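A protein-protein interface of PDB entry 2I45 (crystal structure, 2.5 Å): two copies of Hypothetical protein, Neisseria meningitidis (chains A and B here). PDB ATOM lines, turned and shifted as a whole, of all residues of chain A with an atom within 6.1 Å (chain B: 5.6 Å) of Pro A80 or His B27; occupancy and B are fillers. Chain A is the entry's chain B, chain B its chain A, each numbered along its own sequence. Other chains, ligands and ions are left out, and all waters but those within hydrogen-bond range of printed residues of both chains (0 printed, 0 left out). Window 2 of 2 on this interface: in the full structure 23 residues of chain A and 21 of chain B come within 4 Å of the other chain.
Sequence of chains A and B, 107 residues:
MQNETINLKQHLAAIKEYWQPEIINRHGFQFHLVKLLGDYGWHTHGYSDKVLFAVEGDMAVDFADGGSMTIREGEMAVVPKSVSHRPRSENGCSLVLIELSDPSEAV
His B27 touches Asp A49 (CB to OD1, 3.9 Å).
CE2 of Phe B29 touches CB of Asp A49, at 3.1 Å.
Lys A50 touches Phe B29.
Val A78 touches Arg B26.
Pro A80 touches His B27 (CG to CE1, 3.5 Å).
No position is printed for both chains.
Of the 6 pairs that touch across the chains among the printed residues, none has its exchanged pair printed and touching as well.
Printed residues of chain B that touch a printed residue of chain A: Arg B26, His B27, Gly B28 and Phe B29.
Hydrophobic or aromatic side chains of chain A that line the printed part of chain B: Val A78 and Pro A80.
O of Lys A50 lies within hydrogen-bond range of N of Val A79 (2.8 Å).
The side-chain carboxylate of Asp A49 lies within hydrogen-bond range of the backbone NH of Lys A81 (2.7 Å).
Printed residues of chain B within 4 Å of Lys A50: Phe B29.
Val A79 touches none of the printed residues of chain B.
Pro A80 touches just one residue of chain B: His B27 (3.5 Å).
Of the printed residues of chain A, Arg B26 touches Val A78.
Of chain A, only Asp A49 and Pro A80 come within 4 Å of His B27.
Of the printed residues of chain A, Phe B29 touches Asp A49 (3.1 Å) and Lys A50 (3.9 Å).
The nearest printed residue of chain B that does not touch Pro A80 is Phe B29 (6.6 Å).
The nearest printed residue of chain B that does not touch Asp A49 is Arg B26 (5.6 Å).
The backbone NH (N) of Gly B28 is in hydrogen-bond range of the side-chain carboxylate (OD1) of Asp A49 (3.4 Å).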
ATOM      1  N   SER A  48      29.270  22.432  12.350  1.00  0.00           N
ATOM      2  CA  SER A  48      28.847  23.819  12.161  1.00  0.00           C
ATOM      3  C   SER A  48      27.493  23.749  11.446  1.00  0.00           C
ATOM      4  O   SER A  48      27.084  22.663  11.115  1.00  0.00           O
ATOM      5  CB  SER A  48      29.920  24.556  11.357  1.00  0.00           C
ATOM      6  OG  SER A  48      29.730  24.246   9.951  1.00  0.00           O
ATOM      7  N   ASP A  49      26.760  24.842  11.227  1.00  0.00           N
ATOM      8  CA  ASP A  49      25.423  24.681  10.641  1.00  0.00           C
ATOM      9  C   ASP A  49      25.586  24.510   9.179  1.00  0.00           C
ATOM     10  O   ASP A  49      26.610  24.903   8.664  1.00  0.00           O
ATOM     11  CB  ASP A  49      24.486  25.844  10.892  1.00  0.00           C
ATOM     12  CG  ASP A  49      24.180  26.038  12.347  1.00  0.00           C
ATOM     13  OD1 ASP A  49      23.756  27.167  12.705  1.00  0.00           O
ATOM     14  OD2 ASP A  49      24.400  25.101  13.157  1.00  0.00           O
ATOM     15  N   LYS A  50      24.595  23.921   8.514  1.00  0.00           N
ATOM     16  CA  LYS A  50      24.671  23.676   7.067  1.00  0.00           C
ATOM     17  C   LYS A  50      23.390  24.144   6.401  1.00  0.00           C
ATOM     18  O   LYS A  50      22.289  23.956   6.943  1.00  0.00           O
ATOM     19  CB  LYS A  50      24.929  22.182   6.766  1.00  0.00           C
ATOM     20  CG  LYS A  50      26.290  21.596   7.340  1.00  0.00           C
ATOM     21  CD  LYS A  50      26.148  20.074   7.903  1.00  0.00           C
ATOM     22  CE  LYS A  50      26.034  20.001   9.538  1.00  0.00           C
ATOM     23  NZ  LYS A  50      26.276  18.659  10.175  1.00  0.00           N
ATOM     24  N   PHE A  63      14.583  14.152  11.608  1.00  0.00           N
ATOM     25  CA  PHE A  63      15.304  14.469  12.856  1.00  0.00           C
ATOM     26  C   PHE A  63      15.062  13.554  14.098  1.00  0.00           C
ATOM     27  O   PHE A  63      14.036  12.851  14.191  1.00  0.00           O
ATOM     28  CB  PHE A  63      15.016  15.884  13.271  1.00  0.00           C
ATOM     29  CG  PHE A  63      15.372  16.891  12.236  1.00  0.00           C
ATOM     30  CD1 PHE A  63      16.612  17.487  12.236  1.00  0.00           C
ATOM     31  CD2 PHE A  63      14.448  17.263  11.262  1.00  0.00           C
ATOM     32  CE1 PHE A  63      16.942  18.483  11.262  1.00  0.00           C
ATOM     33  CE2 PHE A  63      14.775  18.222  10.275  1.00  0.00           C
ATOM     34  CZ  PHE A  63      16.028  18.827  10.285  1.00  0.00           C
ATOM     35  N   VAL A  78      17.904  24.543   6.699  1.00  0.00           N
ATOM     36  CA  VAL A  78      19.172  24.498   7.367  1.00  0.00           C
ATOM     37  C   VAL A  78      19.259  23.378   8.402  1.00  0.00           C
ATOM     38  O   VAL A  78      18.347  23.176   9.176  1.00  0.00           O
ATOM     39  CB  VAL A  78      19.607  25.899   7.879  1.00  0.00           C
ATOM     40  CG1 VAL A  78      18.479  26.891   7.744  1.00  0.00           C
ATOM     41  CG2 VAL A  78      20.196  25.855   9.301  1.00  0.00           C
ATOM     42  N   VAL A  79      20.340  22.616   8.390  1.00  0.00           N
ATOM     43  CA  VAL A  79      20.482  21.620   9.408  1.00  0.00           C
ATOM     44  C   VAL A  79      21.475  22.059  10.434  1.00  0.00           C
ATOM     45  O   VAL A  79      22.641  22.149  10.158  1.00  0.00           O
ATOM     46  CB  VAL A  79      20.875  20.296   8.855  1.00  0.00           C
ATOM     47  CG1 VAL A  79      21.273  19.360  10.015  1.00  0.00           C
ATOM     48  CG2 VAL A  79      19.721  19.760   8.105  1.00  0.00           C
ATOM     49  N   PRO A  80      20.992  22.393  11.622  1.00  0.00           N
ATOM     50  CA  PRO A  80      21.914  22.968  12.585  1.00  0.00           C
ATOM     51  C   PRO A  80      22.872  21.920  13.081  1.00  0.00           C
ATOM     52  O   PRO A  80      22.552  20.693  13.097  1.00  0.00           O
ATOM     53  CB  PRO A  80      21.025  23.431  13.739  1.00  0.00           C
ATOM     54  CG  PRO A  80      19.709  22.741  13.568  1.00  0.00           C
ATOM     55  CD  PRO A  80      19.593  22.306  12.104  1.00  0.00           C
ATOM     56  N   LYS A  81      24.056  22.406  13.528  1.00  0.00           N
ATOM     57  CA  LYS A  81      25.108  21.470  14.006  1.00  0.00           C
ATOM     58  C   LYS A  81      24.449  20.773  15.144  1.00  0.00           C
ATOM     59  O   LYS A  81      23.530  21.330  15.702  1.00  0.00           O
ATOM     60  CB  LYS A  81      26.190  22.280  14.583  1.00  0.00           C
ATOM     61  N   SER A  82      24.857  19.525  15.449  1.00  0.00           N
ATOM     62  CA  SER A  82      24.538  18.802  16.721  1.00  0.00           C
ATOM     63  C   SER A  82      23.071  18.414  16.936  1.00  0.00           C
ATOM     64  O   SER A  82      22.492  18.454  18.066  1.00  0.00           O
ATOM     65  CB  SER A  82      25.016  19.686  17.855  1.00  0.00           C
ATOM     66  OG  SER A  82      26.100  20.572  17.385  1.00  0.00           O
ATOM     67  N   VAL A  83      22.517  18.056  15.802  1.00  0.00           N
ATOM     68  CA  VAL A  83      21.199  17.596  15.669  1.00  0.00           C
ATOM     69  C   VAL A  83      21.483  16.383  14.807  1.00  0.00           C
ATOM     70  O   VAL A  83      21.983  16.509  13.693  1.00  0.00           O
ATOM     71  CB  VAL A  83      20.419  18.722  14.981  1.00  0.00           C
ATOM     72  CG1 VAL A  83      19.489  18.211  13.843  1.00  0.00           C
ATOM     73  CG2 VAL A  83      19.679  19.536  16.027  1.00  0.00           C
ATOM     74  N   SER A  84      21.220  15.199  15.321  1.00  0.00           N
ATOM     75  CA  SER A  84      21.315  14.001  14.521  1.00  0.00           C
ATOM     76  C   SER A  84      20.136  13.950  13.555  1.00  0.00           C
ATOM     77  O   SER A  84      19.013  14.180  13.970  1.00  0.00           O
ATOM     78  CB  SER A  84      21.324  12.818  15.460  1.00  0.00           C
ATOM     79  OG  SER A  84      20.482  11.741  15.037  1.00  0.00           O
ATOM     80  N   HIS A  85      20.400  13.676  12.273  1.00  0.00           N
ATOM     81  CA  HIS A  85      19.391  13.690  11.269  1.00  0.00           C
ATOM     82  C   HIS A  85      19.734  12.664  10.242  1.00  0.00           C
ATOM     83  O   HIS A  85      20.868  12.190  10.123  1.00  0.00           O
ATOM     84  CB  HIS A  85      19.359  15.027  10.560  1.00  0.00           C
ATOM     85  CG  HIS A  85      20.686  15.422   9.977  1.00  0.00           C
ATOM     86  ND1 HIS A  85      21.743  15.857  10.759  1.00  0.00           N
ATOM     87  CD2 HIS A  85      21.141  15.423   8.700  1.00  0.00           C
ATOM     88  CE1 HIS A  85      22.783  16.119   9.984  1.00  0.00           C
ATOM     89  NE2 HIS A  85      22.444  15.852   8.737  1.00  0.00           N
ATOM     90  N   ASN B  25      15.229  34.527   8.818  1.00  0.00           N
ATOM     91  CA  ASN B  25      16.192  33.953   9.779  1.00  0.00           C
ATOM     92  C   ASN B  25      15.976  32.498  10.079  1.00  0.00           C
ATOM     93  O   ASN B  25      14.844  31.989  10.134  1.00  0.00           O
ATOM     94  CB  ASN B  25      16.310  34.773  11.081  1.00  0.00           C
ATOM     95  CG  ASN B  25      17.510  35.722  11.058  1.00  0.00           C
ATOM     96  OD1 ASN B  25      17.607  36.580  10.211  1.00  0.00           O
ATOM     97  ND2 ASN B  25      18.432  35.542  11.984  1.00  0.00           N
ATOM     98  N   ARG B  26      17.093  31.826  10.277  1.00  0.00           N
ATOM     99  CA  ARG B  26      17.070  30.388  10.424  1.00  0.00           C
ATOM    100  C   ARG B  26      18.403  29.954  11.062  1.00  0.00           C
ATOM    101  O   ARG B  26      19.416  29.772  10.398  1.00  0.00           O
ATOM    102  CB  ARG B  26      16.732  29.738   9.050  1.00  0.00           C
ATOM    103  CG  ARG B  26      15.581  28.734   9.121  1.00  0.00           C
ATOM    104  CD  ARG B  26      14.423  29.006   8.149  1.00  0.00           C
ATOM    105  NE  ARG B  26      13.599  30.160   8.544  1.00  0.00           N
ATOM    106  CZ  ARG B  26      12.350  30.391   8.129  1.00  0.00           C
ATOM    107  NH1 ARG B  26      11.723  29.532   7.341  1.00  0.00           N
ATOM    108  NH2 ARG B  26      11.713  31.491   8.516  1.00  0.00           N
ATOM    109  N   HIS B  27      18.396  29.849  12.380  1.00  0.00           N
ATOM    110  CA  HIS B  27      19.588  29.449  13.148  1.00  0.00           C
ATOM    111  C   HIS B  27      20.740  30.468  13.001  1.00  0.00           C
ATOM    112  O   HIS B  27      20.505  31.667  13.178  1.00  0.00           O
ATOM    113  CB  HIS B  27      19.995  28.001  12.819  1.00  0.00           C
ATOM    114  CG  HIS B  27      19.000  26.975  13.283  1.00  0.00           C
ATOM    115  ND1 HIS B  27      19.020  26.437  14.558  1.00  0.00           N
ATOM    116  CD2 HIS B  27      17.957  26.389  12.645  1.00  0.00           C
ATOM    117  CE1 HIS B  27      18.038  25.560  14.681  1.00  0.00           C
ATOM    118  NE2 HIS B  27      17.378  25.516  13.535  1.00  0.00           N
ATOM    119  N   GLY B  28      21.959  30.025  12.684  1.00  0.00           N
ATOM    120  CA  GLY B  28      23.093  30.948  12.465  1.00  0.00           C
ATOM    121  C   GLY B  28      22.954  31.836  11.238  1.00  0.00           C
ATOM    122  O   GLY B  28      23.558  32.911  11.172  1.00  0.00           O
ATOM    123  N   PHE B  29      22.121  31.400  10.292  1.00  0.00           N
ATOM    124  CA  PHE B  29      21.998  32.007   8.960  1.00  0.00           C
ATOM    125  C   PHE B  29      20.886  33.043   8.754  1.00  0.00           C
ATOM    126  O   PHE B  29      19.719  32.790   9.092  1.00  0.00           O
ATOM    127  CB  PHE B  29      21.833  30.898   7.910  1.00  0.00           C
ATOM    128  CG  PHE B  29      22.977  29.941   7.878  1.00  0.00           C
ATOM    129  CD1 PHE B  29      24.152  30.259   7.213  1.00  0.00           C
ATOM    130  CD2 PHE B  29      22.904  28.727   8.544  1.00  0.00           C
ATOM    131  CE1 PHE B  29      25.240  29.352   7.205  1.00  0.00           C
ATOM    132  CE2 PHE B  29      23.978  27.820   8.533  1.00  0.00           C
ATOM    133  CZ  PHE B  29      25.146  28.135   7.873  1.00  0.00           C
